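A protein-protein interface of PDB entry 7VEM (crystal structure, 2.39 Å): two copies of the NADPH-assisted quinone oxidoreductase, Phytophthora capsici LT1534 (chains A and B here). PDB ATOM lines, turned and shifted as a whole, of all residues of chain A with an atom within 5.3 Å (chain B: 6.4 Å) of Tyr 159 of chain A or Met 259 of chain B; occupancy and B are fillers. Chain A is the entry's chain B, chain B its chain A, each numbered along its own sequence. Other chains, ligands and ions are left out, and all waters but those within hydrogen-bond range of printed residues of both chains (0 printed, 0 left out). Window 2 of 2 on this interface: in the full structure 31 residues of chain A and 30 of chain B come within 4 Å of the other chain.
Tyr 159 of chain B touches its own counterpart, Tyr 159 of chain A. Tyr 159 of chain A touches Val 160 of chain B, and with the chains exchanged Val 160 of chain A touches Tyr 159 of chain B. Tyr 159 of chain A touches Met 259 of chain B, and with the chains exchanged Met 259 of chain A touches Tyr 159 of chain B. Val 160 of chain B touches its own counterpart, Val 160 of chain A. Of the 8 pairs that touch across the chains among the printed residues, 6 have their exchanged pair printed and touching as well.
Among the printed residues, merely in contact across the chains: Tyr 159 of chain A with Tyr 159 of chain B (3.8 Å), Tyr 159 of chain A with Val 160 of chain B (3.5 Å), Tyr 159 of chain A with Met 259 of chain B (3.5 Å), Val 160 of chain A with Tyr 159 of chain B (3.4 Å), Val 160 of chain A with Val 160 of chain B (3.8 Å), Met 259 of chain A with Tyr 159 of chain B (3.5 Å), Arg 289 of chain A with Cys 286 of chain B (3.8 Å) and Arg 289 of chain A with Ala 287 of chain B (3.9 Å).
Of chain B, only Tyr 159 (3.8 Å), Val 160 (3.5 Å) and Met 259 (3.5 Å) come within 4 Å of Tyr 159 of chain A. Printed residues of chain A within 4 Å of Ala 287 of chain B: Arg 289 (3.9 Å). Of the printed residues of chain B, Arg 289 of chain A touches Cys 286 and Ala 287. Of the printed residues of chain A, Cys 286 of chain B touches Arg 289. Of the printed residues of chain B, Met 259 of chain A touches Tyr 159 (3.5 Å). Printed residues of chain B within 4 Å of Val 160 of chain A: Tyr 159 (3.4 Å) and Val 160 (3.8 Å). Ile 260 of chain B touches none of the printed residues of chain A. The nearest printed residue of chain A that does not touch Met 259 of chain B is Met 259 of chain A (6.3 Å). The nearest printed residue of chain A that does not touch Ala 287 of chain B is Tyr 159 of chain A (4.2 Å).
Of the 8 printed residues of chain A, 4 touch a printed residue of chain B. Printed residues of chain A that touch a printed residue of chain B: Tyr 159, Val 160, Met 259 and Arg 289. Hydrophobic or aromatic side chains of chain A that line the printed part of chain B: Tyr 159, Val 160 and Met 259. Of the 20 printed residues of chain B, 5 touch a printed residue of chain A.
OH of Tyr 237 of chain B lies within hydrogen-bond range of O of Val 160 of chain B (2.7 Å). The backbone carbonyl oxygen of Asp 236 of chain B is in hydrogen-bond range of the backbone NH of Met 259 of chain B. The backbone NH (N) of Val 238 of chain B is in hydrogen-bond range of the backbone carbonyl oxygen (O) of Met 259 of chain B. O of Gly 258 of chain B is in hydrogen-bond range of N of Ala 287 of chain B, 2.8 Å away. The backbone carbonyl oxygen (O) of Ala 287 of chain B is in hydrogen-bond range of the backbone NH (N) of Ile 260 of chain B (2.9 Å). The side-chain amide oxygen of Asn 154 of chain A lies within hydrogen-bond range of the guanidinium group of Arg 289 of chain A (2.8 Å).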
ATOM      1  N   ASN A 154      30.378  -3.518  -1.975  1.00  0.00           N
ATOM      2  CA  ASN A 154      29.176  -3.877  -2.685  1.00  0.00           C
ATOM      3  C   ASN A 154      28.246  -2.662  -2.776  1.00  0.00           C
ATOM      4  O   ASN A 154      27.706  -2.374  -3.854  1.00  0.00           O
ATOM      5  CB  ASN A 154      28.460  -5.057  -2.019  1.00  0.00           C
ATOM      6  CG  ASN A 154      27.350  -5.623  -2.883  1.00  0.00           C
ATOM      7  OD1 ASN A 154      27.139  -5.136  -3.993  1.00  0.00           O
ATOM      8  ND2 ASN A 154      26.657  -6.674  -2.391  1.00  0.00           N
ATOM      9  N   TYR A 157      30.258   0.040  -5.125  1.00  0.00           N
ATOM     10  CA  TYR A 157      30.819  -0.383  -6.418  1.00  0.00           C
ATOM     11  C   TYR A 157      30.145  -1.602  -7.027  1.00  0.00           C
ATOM     12  O   TYR A 157      30.509  -1.994  -8.090  1.00  0.00           O
ATOM     13  CB  TYR A 157      32.328  -0.637  -6.249  1.00  0.00           C
ATOM     14  CG  TYR A 157      33.039   0.648  -6.055  1.00  0.00           C
ATOM     15  CD1 TYR A 157      33.179   1.540  -7.116  1.00  0.00           C
ATOM     16  CD2 TYR A 157      33.537   1.026  -4.809  1.00  0.00           C
ATOM     17  CE1 TYR A 157      33.825   2.763  -6.952  1.00  0.00           C
ATOM     18  CE2 TYR A 157      34.194   2.251  -4.629  1.00  0.00           C
ATOM     19  CZ  TYR A 157      34.340   3.115  -5.708  1.00  0.00           C
ATOM     20  OH  TYR A 157      34.958   4.345  -5.559  1.00  0.00           O
ATOM     21  N   GLY A 158      29.133  -2.175  -6.380  1.00  0.00           N
ATOM     22  CA  GLY A 158      28.538  -3.409  -6.829  1.00  0.00           C
ATOM     23  C   GLY A 158      27.376  -3.245  -7.755  1.00  0.00           C
ATOM     24  O   GLY A 158      27.035  -4.170  -8.459  1.00  0.00           O
ATOM     25  N   TYR A 159      26.758  -2.065  -7.745  1.00  0.00           N
ATOM     26  CA  TYR A 159      25.610  -1.754  -8.581  1.00  0.00           C
ATOM     27  C   TYR A 159      25.947  -0.585  -9.497  1.00  0.00           C
ATOM     28  O   TYR A 159      26.511  -0.818 -10.545  1.00  0.00           O
ATOM     29  CB  TYR A 159      24.385  -1.516  -7.695  1.00  0.00           C
ATOM     30  CG  TYR A 159      23.062  -1.804  -8.365  1.00  0.00           C
ATOM     31  CD1 TYR A 159      22.817  -3.038  -8.985  1.00  0.00           C
ATOM     32  CD2 TYR A 159      22.061  -0.867  -8.362  1.00  0.00           C
ATOM     33  CE1 TYR A 159      21.599  -3.315  -9.560  1.00  0.00           C
ATOM     34  CE2 TYR A 159      20.832  -1.141  -8.929  1.00  0.00           C
ATOM     35  CZ  TYR A 159      20.598  -2.345  -9.520  1.00  0.00           C
ATOM     36  OH  TYR A 159      19.363  -2.559 -10.069  1.00  0.00           O
ATOM     37  N   VAL A 160      25.626   0.657  -9.171  1.00  0.00           N
ATOM     38  CA  VAL A 160      26.103   1.744  -9.977  1.00  0.00           C
ATOM     39  C   VAL A 160      27.288   2.291  -9.181  1.00  0.00           C
ATOM     40  O   VAL A 160      27.186   2.585  -7.977  1.00  0.00           O
ATOM     41  CB  VAL A 160      25.042   2.838 -10.258  1.00  0.00           C
ATOM     42  CG1 VAL A 160      25.614   3.910 -11.205  1.00  0.00           C
ATOM     43  CG2 VAL A 160      23.781   2.248 -10.885  1.00  0.00           C
ATOM     44  N   PRO A 161      28.432   2.431  -9.856  1.00  0.00           N
ATOM     45  CA  PRO A 161      29.643   2.730  -9.079  1.00  0.00           C
ATOM     46  C   PRO A 161      29.784   4.214  -8.647  1.00  0.00           C
ATOM     47  O   PRO A 161      29.413   5.115  -9.361  1.00  0.00           O
ATOM     48  CB  PRO A 161      30.756   2.283 -10.026  1.00  0.00           C
ATOM     49  CG  PRO A 161      30.173   2.507 -11.437  1.00  0.00           C
ATOM     50  CD  PRO A 161      28.712   2.226 -11.299  1.00  0.00           C
ATOM     51  N   MET A 259      21.980   6.972  -4.148  1.00  0.00           N
ATOM     52  CA  MET A 259      21.778   5.551  -3.737  1.00  0.00           C
ATOM     53  C   MET A 259      21.784   5.423  -2.198  1.00  0.00           C
ATOM     54  O   MET A 259      22.680   5.942  -1.518  1.00  0.00           O
ATOM     55  CB  MET A 259      22.814   4.612  -4.428  1.00  0.00           C
ATOM     56  CG  MET A 259      22.912   3.184  -3.841  1.00  0.00           C
ATOM     57  SD  MET A 259      21.303   2.374  -3.814  1.00  0.00           S
ATOM     58  CE  MET A 259      21.167   1.775  -5.522  1.00  0.00           C
ATOM     59  N   ARG A 289      18.625   0.120  -2.038  1.00  0.00           N
ATOM     60  CA  ARG A 289      19.066  -1.225  -2.373  1.00  0.00           C
ATOM     61  C   ARG A 289      19.471  -2.046  -1.116  1.00  0.00           C
ATOM     62  O   ARG A 289      20.347  -1.633  -0.337  1.00  0.00           O
ATOM     63  CB  ARG A 289      20.213  -1.104  -3.332  1.00  0.00           C
ATOM     64  CG  ARG A 289      20.726  -2.411  -3.893  1.00  0.00           C
ATOM     65  CD  ARG A 289      22.080  -2.140  -4.488  1.00  0.00           C
ATOM     66  NE  ARG A 289      22.776  -3.377  -4.716  1.00  0.00           N
ATOM     67  CZ  ARG A 289      24.081  -3.575  -4.585  1.00  0.00           C
ATOM     68  NH1 ARG A 289      24.939  -2.621  -4.252  1.00  0.00           N
ATOM     69  NH2 ARG A 289      24.549  -4.785  -4.857  1.00  0.00           N
ATOM     70  N   ALA B 155      13.232   3.623 -16.431  1.00  0.00           N
ATOM     71  CA  ALA B 155      13.164   2.540 -15.494  1.00  0.00           C
ATOM     72  C   ALA B 155      14.023   1.354 -15.958  1.00  0.00           C
ATOM     73  O   ALA B 155      14.708   0.785 -15.156  1.00  0.00           O
ATOM     74  CB  ALA B 155      11.716   2.094 -15.364  1.00  0.00           C
ATOM     75  N   TYR B 159      19.292   3.411 -15.206  1.00  0.00           N
ATOM     76  CA  TYR B 159      20.138   3.143 -14.072  1.00  0.00           C
ATOM     77  C   TYR B 159      21.019   1.890 -14.310  1.00  0.00           C
ATOM     78  O   TYR B 159      22.139   2.051 -14.727  1.00  0.00           O
ATOM     79  CB  TYR B 159      19.295   3.084 -12.815  1.00  0.00           C
ATOM     80  CG  TYR B 159      20.046   3.359 -11.544  1.00  0.00           C
ATOM     81  CD1 TYR B 159      20.660   4.600 -11.327  1.00  0.00           C
ATOM     82  CD2 TYR B 159      20.088   2.421 -10.521  1.00  0.00           C
ATOM     83  CE1 TYR B 159      21.325   4.878 -10.153  1.00  0.00           C
ATOM     84  CE2 TYR B 159      20.784   2.677  -9.331  1.00  0.00           C
ATOM     85  CZ  TYR B 159      21.396   3.892  -9.147  1.00  0.00           C
ATOM     86  OH  TYR B 159      22.053   4.144  -7.965  1.00  0.00           O
ATOM     87  N   VAL B 160      20.555   0.670 -14.035  1.00  0.00           N
ATOM     88  CA  VAL B 160      21.230  -0.547 -14.509  1.00  0.00           C
ATOM     89  C   VAL B 160      20.365  -1.093 -15.664  1.00  0.00           C
ATOM     90  O   VAL B 160      19.167  -1.237 -15.520  1.00  0.00           O
ATOM     91  CB  VAL B 160      21.448  -1.561 -13.383  1.00  0.00           C
ATOM     92  CG1 VAL B 160      22.218  -2.770 -13.910  1.00  0.00           C
ATOM     93  CG2 VAL B 160      22.261  -0.925 -12.253  1.00  0.00           C
ATOM     94  N   ALA B 235      10.991 -11.859 -10.845  1.00  0.00           N
ATOM     95  CA  ALA B 235      11.155 -10.936 -11.922  1.00  0.00           C
ATOM     96  C   ALA B 235      12.399 -10.062 -11.732  1.00  0.00           C
ATOM     97  O   ALA B 235      12.751  -9.712 -10.604  1.00  0.00           O
ATOM     98  CB  ALA B 235       9.920 -10.068 -12.008  1.00  0.00           C
ATOM     99  N   ASP B 236      13.062  -9.735 -12.834  1.00  0.00           N
ATOM    100  CA  ASP B 236      14.280  -8.893 -12.808  1.00  0.00           C
ATOM    101  C   ASP B 236      13.957  -7.406 -12.659  1.00  0.00           C
ATOM    102  O   ASP B 236      14.703  -6.702 -11.982  1.00  0.00           O
ATOM    103  CB  ASP B 236      15.083  -9.092 -14.077  1.00  0.00           C
ATOM    104  CG  ASP B 236      15.527 -10.514 -14.245  1.00  0.00           C
ATOM    105  OD1 ASP B 236      16.429 -10.969 -13.514  1.00  0.00           O
ATOM    106  OD2 ASP B 236      14.949 -11.210 -15.079  1.00  0.00           O
ATOM    107  N   TYR B 237      12.875  -6.943 -13.329  1.00  0.00           N
ATOM    108  CA  TYR B 237      12.339  -5.565 -13.182  1.00  0.00           C
ATOM    109  C   TYR B 237      10.852  -5.575 -12.837  1.00  0.00           C
ATOM    110  O   TYR B 237      10.107  -6.375 -13.376  1.00  0.00           O
ATOM    111  CB  TYR B 237      12.541  -4.726 -14.445  1.00  0.00           C
ATOM    112  CG  TYR B 237      13.968  -4.449 -14.775  1.00  0.00           C
ATOM    113  CD1 TYR B 237      14.790  -5.435 -15.423  1.00  0.00           C
ATOM    114  CD2 TYR B 237      14.535  -3.221 -14.481  1.00  0.00           C
ATOM    115  CE1 TYR B 237      16.136  -5.186 -15.721  1.00  0.00           C
ATOM    116  CE2 TYR B 237      15.874  -2.954 -14.777  1.00  0.00           C
ATOM    117  CZ  TYR B 237      16.671  -3.937 -15.406  1.00  0.00           C
ATOM    118  OH  TYR B 237      17.993  -3.641 -15.688  1.00  0.00           O
ATOM    119  N   VAL B 238      10.428  -4.691 -11.938  1.00  0.00           N
ATOM    120  CA  VAL B 238       9.003  -4.490 -11.675  1.00  0.00           C
ATOM    121  C   VAL B 238       8.704  -3.026 -11.946  1.00  0.00           C
ATOM    122  O   VAL B 238       9.333  -2.132 -11.353  1.00  0.00           O
ATOM    123  CB  VAL B 238       8.596  -4.843 -10.227  1.00  0.00           C
ATOM    124  CG1 VAL B 238       7.109  -4.583  -9.976  1.00  0.00           C
ATOM    125  CG2 VAL B 238       8.902  -6.305  -9.938  1.00  0.00           C
ATOM    126  N   ILE B 239       7.758  -2.792 -12.854  1.00  0.00           N
ATOM    127  CA  ILE B 239       7.247  -1.444 -13.154  1.00  0.00           C
ATOM    128  C   ILE B 239       6.097  -1.130 -12.182  1.00  0.00           C
ATOM    129  O   ILE B 239       4.912  -1.449 -12.460  1.00  0.00           O
ATOM    130  CB  ILE B 239       6.804  -1.359 -14.624  1.00  0.00           C
ATOM    131  CG1 ILE B 239       7.953  -1.766 -15.554  1.00  0.00           C
ATOM    132  CG2 ILE B 239       6.319   0.035 -14.986  1.00  0.00           C
ATOM    133  CD1 ILE B 239       9.325  -1.225 -15.193  1.00  0.00           C
ATOM    134  N   THR B 254      10.301 -10.030  -6.794  1.00  0.00           N
ATOM    135  CA  THR B 254      11.521  -9.573  -7.457  1.00  0.00           C
ATOM    136  C   THR B 254      12.690 -10.504  -7.132  1.00  0.00           C
ATOM    137  O   THR B 254      12.813 -10.934  -6.012  1.00  0.00           O
ATOM    138  CB  THR B 254      11.852  -8.143  -7.022  1.00  0.00           C
ATOM    139  OG1 THR B 254      10.728  -7.340  -7.290  1.00  0.00           O
ATOM    140  CG2 THR B 254      13.046  -7.566  -7.769  1.00  0.00           C
ATOM    141  N   ALA B 255      13.499 -10.836  -8.136  1.00  0.00           N
ATOM    142  CA  ALA B 255      14.749 -11.569  -7.960  1.00  0.00           C
ATOM    143  C   ALA B 255      15.715 -10.841  -7.058  1.00  0.00           C
ATOM    144  O   ALA B 255      15.618  -9.646  -6.909  1.00  0.00           O
ATOM    145  CB  ALA B 255      15.428 -11.758  -9.316  1.00  0.00           C
ATOM    146  N   GLY B 257      19.076  -9.015  -6.550  1.00  0.00           N
ATOM    147  CA  GLY B 257      19.709  -8.235  -7.603  1.00  0.00           C
ATOM    148  C   GLY B 257      18.747  -7.561  -8.606  1.00  0.00           C
ATOM    149  O   GLY B 257      19.217  -6.909  -9.515  1.00  0.00           O
ATOM    150  N   GLY B 258      17.423  -7.663  -8.421  1.00  0.00           N
ATOM    151  CA  GLY B 258      16.496  -7.048  -9.327  1.00  0.00           C
ATOM    152  C   GLY B 258      16.204  -5.622  -8.928  1.00  0.00           C
ATOM    153  O   GLY B 258      16.641  -5.136  -7.859  1.00  0.00           O
ATOM    154  N   MET B 259      15.385  -4.995  -9.763  1.00  0.00           N
ATOM    155  CA  MET B 259      15.068  -3.559  -9.708  1.00  0.00           C
ATOM    156  C   MET B 259      13.560  -3.373  -9.689  1.00  0.00           C
ATOM    157  O   MET B 259      12.864  -3.896 -10.563  1.00  0.00           O
ATOM    158  CB  MET B 259      15.654  -2.837 -10.952  1.00  0.00           C
ATOM    159  CG  MET B 259      15.107  -1.418 -11.222  1.00  0.00           C
ATOM    160  SD  MET B 259      15.368  -0.321  -9.799  1.00  0.00           S
ATOM    161  CE  MET B 259      17.079   0.126 -10.067  1.00  0.00           C
ATOM    162  N   ILE B 260      13.063  -2.616  -8.713  1.00  0.00           N
ATOM    163  CA  ILE B 260      11.681  -2.171  -8.700  1.00  0.00           C
ATOM    164  C   ILE B 260      11.671  -0.677  -8.998  1.00  0.00           C
ATOM    165  O   ILE B 260      12.112   0.145  -8.178  1.00  0.00           O
ATOM    166  CB  ILE B 260      10.993  -2.486  -7.371  1.00  0.00           C
ATOM    167  CG1 ILE B 260      11.084  -3.986  -7.084  1.00  0.00           C
ATOM    168  CG2 ILE B 260       9.493  -2.128  -7.388  1.00  0.00           C
ATOM    169  CD1 ILE B 260      10.662  -4.297  -5.687  1.00  0.00           C
ATOM    170  N   ALA B 261      11.191  -0.347 -10.195  1.00  0.00           N
ATOM    171  CA  ALA B 261      11.040   1.022 -10.647  1.00  0.00           C
ATOM    172  C   ALA B 261       9.727   1.543 -10.092  1.00  0.00           C
ATOM    173  O   ALA B 261       8.650   1.197 -10.597  1.00  0.00           O
ATOM    174  CB  ALA B 261      11.052   1.109 -12.182  1.00  0.00           C
ATOM    175  N   VAL B 262       9.841   2.344  -9.030  1.00  0.00           N
ATOM    176  CA  VAL B 262       8.708   3.008  -8.395  1.00  0.00           C
ATOM    177  C   VAL B 262       8.340   4.234  -9.206  1.00  0.00           C
ATOM    178  O   VAL B 262       9.153   5.174  -9.371  1.00  0.00           O
ATOM    179  CB  VAL B 262       9.015   3.405  -6.928  1.00  0.00           C
ATOM    180  CG1 VAL B 262       7.879   4.249  -6.347  1.00  0.00           C
ATOM    181  CG2 VAL B 262       9.235   2.146  -6.074  1.00  0.00           C
ATOM    182  N   CYS B 286      17.136  -6.765  -3.196  1.00  0.00           N
ATOM    183  CA  CYS B 286      16.726  -6.120  -4.449  1.00  0.00           C
ATOM    184  C   CYS B 286      16.674  -4.657  -4.224  1.00  0.00           C
ATOM    185  O   CYS B 286      16.772  -4.198  -3.095  1.00  0.00           O
ATOM    186  CB  CYS B 286      15.381  -6.654  -4.919  1.00  0.00           C
ATOM    187  SG  CYS B 286      13.993  -6.131  -3.931  1.00  0.00           S
ATOM    188  N   ALA B 287      16.576  -3.933  -5.325  1.00  0.00           N
ATOM    189  CA  ALA B 287      16.610  -2.465  -5.304  1.00  0.00           C
ATOM    190  C   ALA B 287      15.225  -1.833  -5.579  1.00  0.00           C
ATOM    191  O   ALA B 287      14.341  -2.460  -6.164  1.00  0.00           O
ATOM    192  CB  ALA B 287      17.636  -1.963  -6.302  1.00  0.00           C
ATOM    193  N   LEU B 288      15.024  -0.623  -5.069  1.00  0.00           N
ATOM    194  CA  LEU B 288      13.877   0.205  -5.433  1.00  0.00           C
ATOM    195  C   LEU B 288      14.419   1.505  -5.937  1.00  0.00           C
ATOM    196  O   LEU B 288      15.390   2.000  -5.386  1.00  0.00           O
ATOM    197  CB  LEU B 288      12.989   0.540  -4.256  1.00  0.00           C
ATOM    198  CG  LEU B 288      12.044  -0.542  -3.768  1.00  0.00           C
ATOM    199  CD1 LEU B 288      12.829  -1.630  -3.027  1.00  0.00           C
ATOM    200  CD2 LEU B 288      10.990   0.057  -2.860  1.00  0.00           C
ATOM    201  N   ARG B 289      13.768   2.086  -6.930  1.00  0.00           N
ATOM    202  CA  ARG B 289      14.187   3.368  -7.433  1.00  0.00           C
ATOM    203  C   ARG B 289      13.000   4.228  -7.805  1.00  0.00           C
ATOM    204  O   ARG B 289      12.128   3.792  -8.548  1.00  0.00           O
ATOM    205  CB  ARG B 289      15.124   3.147  -8.611  1.00  0.00           C
ATOM    206  CG  ARG B 289      15.689   4.415  -9.259  1.00  0.00           C
ATOM    207  CD  ARG B 289      16.417   4.022 -10.542  1.00  0.00           C
ATOM    208  NE  ARG B 289      16.637   5.179 -11.364  1.00  0.00           N
ATOM    209  CZ  ARG B 289      16.325   5.319 -12.651  1.00  0.00           C
ATOM    210  NH1 ARG B 289      15.777   4.341 -13.388  1.00  0.00           N
ATOM    211  NH2 ARG B 289      16.600   6.491 -13.225  1.00  0.00           N
